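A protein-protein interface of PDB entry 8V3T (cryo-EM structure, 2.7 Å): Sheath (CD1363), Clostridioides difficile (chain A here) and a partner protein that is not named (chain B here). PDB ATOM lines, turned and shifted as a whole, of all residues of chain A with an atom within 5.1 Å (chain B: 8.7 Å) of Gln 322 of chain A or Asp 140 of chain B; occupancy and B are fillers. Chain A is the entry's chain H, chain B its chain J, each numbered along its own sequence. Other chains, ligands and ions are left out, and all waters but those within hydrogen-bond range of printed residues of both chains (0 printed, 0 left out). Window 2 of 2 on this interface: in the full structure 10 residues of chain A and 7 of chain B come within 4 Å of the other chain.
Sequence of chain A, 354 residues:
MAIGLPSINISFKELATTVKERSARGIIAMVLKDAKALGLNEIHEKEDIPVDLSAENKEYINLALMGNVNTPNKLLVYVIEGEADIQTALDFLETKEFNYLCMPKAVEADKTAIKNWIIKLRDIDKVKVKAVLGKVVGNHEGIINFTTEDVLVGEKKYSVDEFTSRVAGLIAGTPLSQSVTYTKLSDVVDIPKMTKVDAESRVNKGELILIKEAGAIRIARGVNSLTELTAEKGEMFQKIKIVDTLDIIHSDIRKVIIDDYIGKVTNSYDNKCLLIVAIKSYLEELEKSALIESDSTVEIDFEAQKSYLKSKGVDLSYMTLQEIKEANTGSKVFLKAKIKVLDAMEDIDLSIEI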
ATOM      1  N   TYR A 269     -18.101  15.803  13.749  1.00  0.00           N
ATOM      2  CA  TYR A 269     -19.408  15.813  14.400  1.00  0.00           C
ATOM      3  C   TYR A 269     -20.187  14.527  14.138  1.00  0.00           C
ATOM      4  O   TYR A 269     -20.947  14.077  15.005  1.00  0.00           O
ATOM      5  CB  TYR A 269     -20.206  17.033  13.943  1.00  0.00           C
ATOM      6  CG  TYR A 269     -21.487  17.237  14.708  1.00  0.00           C
ATOM      7  CD1 TYR A 269     -21.475  17.430  16.080  1.00  0.00           C
ATOM      8  CD2 TYR A 269     -22.711  17.238  14.059  1.00  0.00           C
ATOM      9  CE1 TYR A 269     -22.644  17.614  16.785  1.00  0.00           C
ATOM     10  CE2 TYR A 269     -23.884  17.421  14.753  1.00  0.00           C
ATOM     11  CZ  TYR A 269     -23.847  17.609  16.116  1.00  0.00           C
ATOM     12  OH  TYR A 269     -25.018  17.791  16.810  1.00  0.00           O
ATOM     13  N   CYS A 273     -21.809  12.064  16.971  1.00  0.00           N
ATOM     14  CA  CYS A 273     -23.177  11.556  16.998  1.00  0.00           C
ATOM     15  C   CYS A 273     -23.202  10.039  17.135  1.00  0.00           C
ATOM     16  O   CYS A 273     -24.031   9.485  17.869  1.00  0.00           O
ATOM     17  CB  CYS A 273     -23.922  11.995  15.739  1.00  0.00           C
ATOM     18  SG  CYS A 273     -24.182  13.775  15.619  1.00  0.00           S
ATOM     19  N   THR A 320     -25.306  30.951  16.731  1.00  0.00           N
ATOM     20  CA  THR A 320     -26.473  30.154  17.068  1.00  0.00           C
ATOM     21  C   THR A 320     -26.085  29.012  18.004  1.00  0.00           C
ATOM     22  O   THR A 320     -24.918  28.626  18.108  1.00  0.00           O
ATOM     23  CB  THR A 320     -27.126  29.597  15.804  1.00  0.00           C
ATOM     24  OG1 THR A 320     -26.856  30.472  14.702  1.00  0.00           O
ATOM     25  CG2 THR A 320     -28.631  29.479  15.987  1.00  0.00           C
ATOM     26  N   LEU A 321     -27.089  28.475  18.702  1.00  0.00           N
ATOM     27  CA  LEU A 321     -26.854  27.316  19.556  1.00  0.00           C
ATOM     28  C   LEU A 321     -26.368  26.127  18.737  1.00  0.00           C
ATOM     29  O   LEU A 321     -25.427  25.429  19.133  1.00  0.00           O
ATOM     30  CB  LEU A 321     -28.135  26.953  20.308  1.00  0.00           C
ATOM     31  CG  LEU A 321     -28.513  27.777  21.541  1.00  0.00           C
ATOM     32  CD1 LEU A 321     -29.729  27.173  22.227  1.00  0.00           C
ATOM     33  CD2 LEU A 321     -27.351  27.895  22.511  1.00  0.00           C
ATOM     34  N   GLN A 322     -26.996  25.890  17.582  1.00  0.00           N
ATOM     35  CA  GLN A 322     -26.581  24.792  16.717  1.00  0.00           C
ATOM     36  C   GLN A 322     -25.174  25.017  16.179  1.00  0.00           C
ATOM     37  O   GLN A 322     -24.393  24.068  16.052  1.00  0.00           O
ATOM     38  CB  GLN A 322     -27.578  24.627  15.569  1.00  0.00           C
ATOM     39  CG  GLN A 322     -27.252  23.495  14.613  1.00  0.00           C
ATOM     40  CD  GLN A 322     -27.558  22.132  15.201  1.00  0.00           C
ATOM     41  OE1 GLN A 322     -28.425  21.998  16.064  1.00  0.00           O
ATOM     42  NE2 GLN A 322     -26.848  21.113  14.735  1.00  0.00           N
ATOM     43  N   GLU A 323     -24.834  26.267  15.858  1.00  0.00           N
ATOM     44  CA  GLU A 323     -23.486  26.573  15.388  1.00  0.00           C
ATOM     45  C   GLU A 323     -22.446  26.260  16.456  1.00  0.00           C
ATOM     46  O   GLU A 323     -21.372  25.730  16.151  1.00  0.00           O
ATOM     47  CB  GLU A 323     -23.397  28.041  14.971  1.00  0.00           C
ATOM     48  CG  GLU A 323     -23.991  28.347  13.607  1.00  0.00           C
ATOM     49  CD  GLU A 323     -23.092  27.918  12.462  1.00  0.00           C
ATOM     50  OE1 GLU A 323     -21.959  27.465  12.728  1.00  0.00           O
ATOM     51  OE2 GLU A 323     -23.518  28.038  11.294  1.00  0.00           O
ATOM     52  N   ILE A 324     -22.745  26.591  17.712  1.00  0.00           N
ATOM     53  CA  ILE A 324     -21.825  26.285  18.801  1.00  0.00           C
ATOM     54  C   ILE A 324     -21.732  24.780  19.015  1.00  0.00           C
ATOM     55  O   ILE A 324     -20.658  24.246  19.320  1.00  0.00           O
ATOM     56  CB  ILE A 324     -22.260  27.014  20.086  1.00  0.00           C
ATOM     57  CG1 ILE A 324     -22.222  28.528  19.878  1.00  0.00           C
ATOM     58  CG2 ILE A 324     -21.369  26.625  21.252  1.00  0.00           C
ATOM     59  CD1 ILE A 324     -22.552  29.318  21.123  1.00  0.00           C
ATOM     60  N   LYS A 325     -22.852  24.070  18.857  1.00  0.00           N
ATOM     61  CA  LYS A 325     -22.875  22.641  19.152  1.00  0.00           C
ATOM     62  C   LYS A 325     -21.942  21.858  18.233  1.00  0.00           C
ATOM     63  O   LYS A 325     -21.231  20.955  18.688  1.00  0.00           O
ATOM     64  CB  LYS A 325     -24.304  22.111  19.050  1.00  0.00           C
ATOM     65  CG  LYS A 325     -24.396  20.610  18.849  1.00  0.00           C
ATOM     66  CD  LYS A 325     -25.833  20.126  18.929  1.00  0.00           C
ATOM     67  CE  LYS A 325     -26.545  20.703  20.138  1.00  0.00           C
ATOM     68  NZ  LYS A 325     -27.998  20.381  20.123  1.00  0.00           N
ATOM     69  N   GLU A 326     -21.922  22.185  16.940  1.00  0.00           N
ATOM     70  CA  GLU A 326     -21.112  21.450  15.977  1.00  0.00           C
ATOM     71  C   GLU A 326     -19.841  22.194  15.585  1.00  0.00           C
ATOM     72  O   GLU A 326     -19.301  21.952  14.501  1.00  0.00           O
ATOM     73  CB  GLU A 326     -21.929  21.116  14.729  1.00  0.00           C
ATOM     74  CG  GLU A 326     -22.689  22.278  14.132  1.00  0.00           C
ATOM     75  CD  GLU A 326     -23.998  21.849  13.500  1.00  0.00           C
ATOM     76  OE1 GLU A 326     -24.627  20.905  14.020  1.00  0.00           O
ATOM     77  OE2 GLU A 326     -24.398  22.452  12.481  1.00  0.00           O
ATOM     78  N   MET B  10     -36.004  20.776   1.361  1.00  0.00           N
ATOM     79  CA  MET B  10     -34.838  19.904   1.398  1.00  0.00           C
ATOM     80  C   MET B  10     -34.859  18.943   0.217  1.00  0.00           C
ATOM     81  O   MET B  10     -35.885  18.330  -0.091  1.00  0.00           O
ATOM     82  CB  MET B  10     -34.788  19.122   2.711  1.00  0.00           C
ATOM     83  CG  MET B  10     -34.669  19.981   3.956  1.00  0.00           C
ATOM     84  SD  MET B  10     -35.286  19.132   5.420  1.00  0.00           S
ATOM     85  CE  MET B  10     -36.097  20.486   6.260  1.00  0.00           C
ATOM     86  N   SER B  91     -29.573   8.511   9.719  1.00  0.00           N
ATOM     87  CA  SER B  91     -29.789   9.232   8.476  1.00  0.00           C
ATOM     88  C   SER B  91     -29.615  10.726   8.708  1.00  0.00           C
ATOM     89  O   SER B  91     -29.999  11.250   9.757  1.00  0.00           O
ATOM     90  CB  SER B  91     -31.182   8.950   7.908  1.00  0.00           C
ATOM     91  OG  SER B  91     -32.133   9.865   8.415  1.00  0.00           O
ATOM     92  N   LYS B  92     -29.026  11.409   7.728  1.00  0.00           N
ATOM     93  CA  LYS B  92     -28.787  12.843   7.809  1.00  0.00           C
ATOM     94  C   LYS B  92     -29.223  13.500   6.510  1.00  0.00           C
ATOM     95  O   LYS B  92     -28.909  13.004   5.425  1.00  0.00           O
ATOM     96  CB  LYS B  92     -27.312  13.148   8.084  1.00  0.00           C
ATOM     97  CG  LYS B  92     -26.999  14.629   8.180  1.00  0.00           C
ATOM     98  CD  LYS B  92     -25.512  14.878   8.341  1.00  0.00           C
ATOM     99  CE  LYS B  92     -24.861  15.227   7.020  1.00  0.00           C
ATOM    100  NZ  LYS B  92     -23.401  15.468   7.174  1.00  0.00           N
ATOM    101  N   LEU B  93     -29.936  14.617   6.624  1.00  0.00           N
ATOM    102  CA  LEU B  93     -30.394  15.389   5.473  1.00  0.00           C
ATOM    103  C   LEU B  93     -29.990  16.839   5.700  1.00  0.00           C
ATOM    104  O   LEU B  93     -30.589  17.529   6.528  1.00  0.00           O
ATOM    105  CB  LEU B  93     -31.906  15.256   5.291  1.00  0.00           C
ATOM    106  CG  LEU B  93     -32.535  15.833   4.023  1.00  0.00           C
ATOM    107  CD1 LEU B  93     -31.989  15.145   2.786  1.00  0.00           C
ATOM    108  CD2 LEU B  93     -34.046  15.705   4.085  1.00  0.00           C
ATOM    109  N   ASN B  94     -28.975  17.301   4.967  1.00  0.00           N
ATOM    110  CA  ASN B  94     -28.406  18.638   5.171  1.00  0.00           C
ATOM    111  C   ASN B  94     -28.267  19.325   3.813  1.00  0.00           C
ATOM    112  O   ASN B  94     -27.225  19.232   3.159  1.00  0.00           O
ATOM    113  CB  ASN B  94     -27.071  18.552   5.900  1.00  0.00           C
ATOM    114  CG  ASN B  94     -26.536  19.910   6.300  1.00  0.00           C
ATOM    115  OD1 ASN B  94     -27.293  20.861   6.481  1.00  0.00           O
ATOM    116  ND2 ASN B  94     -25.221  20.006   6.440  1.00  0.00           N
ATOM    117  N   TYR B  99     -32.957  25.204   5.606  1.00  0.00           N
ATOM    118  CA  TYR B  99     -32.840  25.943   6.857  1.00  0.00           C
ATOM    119  C   TYR B  99     -31.848  25.291   7.814  1.00  0.00           C
ATOM    120  O   TYR B  99     -31.105  25.993   8.509  1.00  0.00           O
ATOM    121  CB  TYR B  99     -34.219  26.079   7.503  1.00  0.00           C
ATOM    122  CG  TYR B  99     -35.235  26.765   6.612  1.00  0.00           C
ATOM    123  CD1 TYR B  99     -35.895  26.068   5.608  1.00  0.00           C
ATOM    124  CD2 TYR B  99     -35.531  28.112   6.774  1.00  0.00           C
ATOM    125  CE1 TYR B  99     -36.815  26.694   4.789  1.00  0.00           C
ATOM    126  CE2 TYR B  99     -36.455  28.744   5.963  1.00  0.00           C
ATOM    127  CZ  TYR B  99     -37.094  28.029   4.974  1.00  0.00           C
ATOM    128  OH  TYR B  99     -38.013  28.652   4.163  1.00  0.00           O
ATOM    129  N   GLY B 100     -31.819  23.967   7.869  1.00  0.00           N
ATOM    130  CA  GLY B 100     -30.902  23.296   8.766  1.00  0.00           C
ATOM    131  C   GLY B 100     -30.786  21.825   8.442  1.00  0.00           C
ATOM    132  O   GLY B 100     -31.351  21.336   7.463  1.00  0.00           O
ATOM    133  N   ALA B 101     -30.038  21.123   9.284  1.00  0.00           N
ATOM    134  CA  ALA B 101     -29.818  19.693   9.145  1.00  0.00           C
ATOM    135  C   ALA B 101     -30.802  18.916  10.009  1.00  0.00           C
ATOM    136  O   ALA B 101     -31.389  19.450  10.953  1.00  0.00           O
ATOM    137  CB  ALA B 101     -28.382  19.323   9.523  1.00  0.00           C
ATOM    138  N   GLU B 102     -30.987  17.644   9.664  1.00  0.00           N
ATOM    139  CA  GLU B 102     -31.898  16.764  10.388  1.00  0.00           C
ATOM    140  C   GLU B 102     -31.258  15.390  10.511  1.00  0.00           C
ATOM    141  O   GLU B 102     -30.971  14.747   9.498  1.00  0.00           O
ATOM    142  CB  GLU B 102     -33.253  16.669   9.678  1.00  0.00           C
ATOM    143  CG  GLU B 102     -34.331  15.981  10.492  1.00  0.00           C
ATOM    144  CD  GLU B 102     -35.725  16.238   9.953  1.00  0.00           C
ATOM    145  OE1 GLU B 102     -36.300  17.300  10.271  1.00  0.00           O
ATOM    146  OE2 GLU B 102     -36.248  15.380   9.213  1.00  0.00           O
ATOM    147  N   ARG B 103     -31.036  14.945  11.745  1.00  0.00           N
ATOM    148  CA  ARG B 103     -30.423  13.654  12.031  1.00  0.00           C
ATOM    149  C   ARG B 103     -31.398  12.803  12.829  1.00  0.00           C
ATOM    150  O   ARG B 103     -32.013  13.285  13.782  1.00  0.00           O
ATOM    151  CB  ARG B 103     -29.123  13.823  12.817  1.00  0.00           C
ATOM    152  CG  ARG B 103     -27.963  14.365  12.016  1.00  0.00           C
ATOM    153  CD  ARG B 103     -26.662  14.171  12.772  1.00  0.00           C
ATOM    154  NE  ARG B 103     -25.588  15.000  12.241  1.00  0.00           N
ATOM    155  CZ  ARG B 103     -24.520  14.527  11.616  1.00  0.00           C
ATOM    156  NH1 ARG B 103     -24.349  13.229  11.425  1.00  0.00           N
ATOM    157  NH2 ARG B 103     -23.601  15.376  11.170  1.00  0.00           N
ATOM    158  N   ILE B 104     -31.549  11.543  12.440  1.00  0.00           N
ATOM    159  CA  ILE B 104     -32.401  10.613  13.171  1.00  0.00           C
ATOM    160  C   ILE B 104     -31.699   9.268  13.254  1.00  0.00           C
ATOM    161  O   ILE B 104     -31.102   8.803  12.278  1.00  0.00           O
ATOM    162  CB  ILE B 104     -33.796  10.473  12.523  1.00  0.00           C
ATOM    163  CG1 ILE B 104     -34.477  11.838  12.416  1.00  0.00           C
ATOM    164  CG2 ILE B 104     -34.668   9.520  13.320  1.00  0.00           C
ATOM    165  CD1 ILE B 104     -35.835  11.798  11.799  1.00  0.00           C
ATOM    166  N   ALA B 105     -31.762   8.649  14.428  1.00  0.00           N
ATOM    167  CA  ALA B 105     -31.238   7.310  14.645  1.00  0.00           C
ATOM    168  C   ALA B 105     -32.401   6.331  14.702  1.00  0.00           C
ATOM    169  O   ALA B 105     -33.375   6.563  15.424  1.00  0.00           O
ATOM    170  CB  ALA B 105     -30.419   7.240  15.934  1.00  0.00           C
ATOM    171  N   ASP B 137     -34.347   7.993  17.988  1.00  0.00           N
ATOM    172  CA  ASP B 137     -33.860   9.134  18.750  1.00  0.00           C
ATOM    173  C   ASP B 137     -33.746  10.343  17.834  1.00  0.00           C
ATOM    174  O   ASP B 137     -33.457  10.201  16.643  1.00  0.00           O
ATOM    175  CB  ASP B 137     -32.501   8.842  19.398  1.00  0.00           C
ATOM    176  CG  ASP B 137     -32.624   8.015  20.661  1.00  0.00           C
ATOM    177  OD1 ASP B 137     -33.123   8.544  21.674  1.00  0.00           O
ATOM    178  OD2 ASP B 137     -32.219   6.834  20.643  1.00  0.00           O
ATOM    179  N   PHE B 138     -33.970  11.529  18.394  1.00  0.00           N
ATOM    180  CA  PHE B 138     -33.904  12.781  17.652  1.00  0.00           C
ATOM    181  C   PHE B 138     -32.556  13.448  17.895  1.00  0.00           C
ATOM    182  O   PHE B 138     -32.176  13.686  19.045  1.00  0.00           O
ATOM    183  CB  PHE B 138     -35.029  13.731  18.060  1.00  0.00           C
ATOM    184  CG  PHE B 138     -36.379  13.343  17.538  1.00  0.00           C
ATOM    185  CD1 PHE B 138     -36.509  12.710  16.315  1.00  0.00           C
ATOM    186  CD2 PHE B 138     -37.523  13.631  18.263  1.00  0.00           C
ATOM    187  CE1 PHE B 138     -37.753  12.357  15.834  1.00  0.00           C
ATOM    188  CE2 PHE B 138     -38.769  13.282  17.785  1.00  0.00           C
ATOM    189  CZ  PHE B 138     -38.884  12.644  16.570  1.00  0.00           C
ATOM    190  N   LEU B 139     -31.839  13.745  16.815  1.00  0.00           N
ATOM    191  CA  LEU B 139     -30.623  14.544  16.865  1.00  0.00           C
ATOM    192  C   LEU B 139     -30.753  15.690  15.872  1.00  0.00           C
ATOM    193  O   LEU B 139     -31.069  15.464  14.701  1.00  0.00           O
ATOM    194  CB  LEU B 139     -29.389  13.698  16.534  1.00  0.00           C
ATOM    195  CG  LEU B 139     -29.265  12.320  17.192  1.00  0.00           C
ATOM    196  CD1 LEU B 139     -28.448  11.382  16.317  1.00  0.00           C
ATOM    197  CD2 LEU B 139     -28.648  12.426  18.576  1.00  0.00           C
ATOM    198  N   ASP B 140     -30.512  16.915  16.332  1.00  0.00           N
ATOM    199  CA  ASP B 140     -30.476  18.080  15.447  1.00  0.00           C
ATOM    200  C   ASP B 140     -31.771  18.238  14.651  1.00  0.00           C
ATOM    201  O   ASP B 140     -31.755  18.387  13.428  1.00  0.00           O
ATOM    202  CB  ASP B 140     -29.281  18.004  14.497  1.00  0.00           C
ATOM    203  CG  ASP B 140     -27.966  17.889  15.226  1.00  0.00           C
ATOM    204  OD1 ASP B 140     -27.910  18.259  16.417  1.00  0.00           O
ATOM    205  OD2 ASP B 140     -26.987  17.423  14.609  1.00  0.00           O
ATOM    206  N   ILE B 141     -32.910  18.183  15.339  1.00  0.00           N
ATOM    207  CA  ILE B 141     -34.174  18.477  14.675  1.00  0.00           C
ATOM    208  C   ILE B 141     -34.305  19.981  14.461  1.00  0.00           C
ATOM    209  O   ILE B 141     -33.799  20.794  15.245  1.00  0.00           O
ATOM    210  CB  ILE B 141     -35.365  17.922  15.476  1.00  0.00           C
ATOM    211  CG1 ILE B 141     -35.216  18.264  16.959  1.00  0.00           C
ATOM    212  CG2 ILE B 141     -35.507  16.422  15.257  1.00  0.00           C
ATOM    213  CD1 ILE B 141     -36.322  17.714  17.823  1.00  0.00           C
ATOM    214  N   ILE B 142     -34.990  20.357  13.386  1.00  0.00           N
ATOM    215  CA  ILE B 142     -35.147  21.765  13.042  1.00  0.00           C
ATOM    216  C   ILE B 142     -36.332  22.371  13.783  1.00  0.00           C
ATOM    217  O   ILE B 142     -37.487  22.150  13.417  1.00  0.00           O
ATOM    218  CB  ILE B 142     -35.305  21.948  11.525  1.00  0.00           C
ATOM    219  CG1 ILE B 142     -34.113  21.335  10.793  1.00  0.00           C
ATOM    220  CG2 ILE B 142     -35.437  23.420  11.178  1.00  0.00           C
ATOM    221  CD1 ILE B 142     -34.236  21.377   9.294  1.00  0.00           C
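Along chain B the printed residues that touch a printed residue of chain A span positions 103 to 140.
Hydrophobic or aromatic side chains of chain A within 4 Å of the printed part of chain B: Tyr 269.
Among the printed residues, no Asp or Glu carboxylate lies within 4 Å of a Lys or Arg side-chain nitrogen of the other chain.
Tyr 269 of chain A touches Arg 103 of chain B.
Cys 273 of chain A touches Arg 103 of chain B (SG to CD, 3.8 Å).
CD of Lys 325 of chain A touches OD1 of Asp 140 of chain B, at 3.8 Å.
The side-chain amide nitrogen (NE2) of Gln 322 of chain A sits close to the side-chain carboxylate (OD1) of Asp 140 of chain B (3.5 Å).
The side-chain hydroxyl (OH) of Tyr 269 of chain A is in hydrogen-bond range of the side-chain carboxylate (OD1) of Asp 140 of chain B, 3.0 Å away.
Asp 140 of chain B touches just these residues of chain A: Tyr 269, Gln 322 and Lys 325.
Printed residues of chain B within 4 Å of Tyr 269 of chain A: Arg 103 (3.6 Å) and Asp 140 (3.0 Å).
Printed residues of chain A within 4 Å of Arg 103 of chain B: Tyr 269 and Cys 273.
Printed residues of chain B within 4 Å of Lys 325 of chain A: Asp 140 (3.8 Å).
Of the printed residues of chain B, Cys 273 of chain A touches Arg 103.
Glu 102 of chain B touches none of the printed residues of chain A.
The nearest residue of chain A that does not touch Asp 140 of chain B is Glu 326 of chain A (4.2 Å).
The nearest printed residue of chain B that does not touch Lys 325 of chain A is Leu 139 of chain B (6.9 Å).
O of Tyr 269 of chain A lies within hydrogen-bond range of SG of Cys 273 of chain A (3.3 Å).
N of Arg 103 of chain B sits at hydrogen-bond distance from O of Leu 139 of chain B (3.0 Å).
The backbone carbonyl oxygen (O) of Ala 101 of chain B sits close to the backbone carbonyl oxygen (O) of Asp 140 of chain B (2.7 Å).
The side-chain carboxylate (OD2) of Asp 140 of chain B is in salt-bridge range of the guanidinium group (NE) of Arg 103 of chain B.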
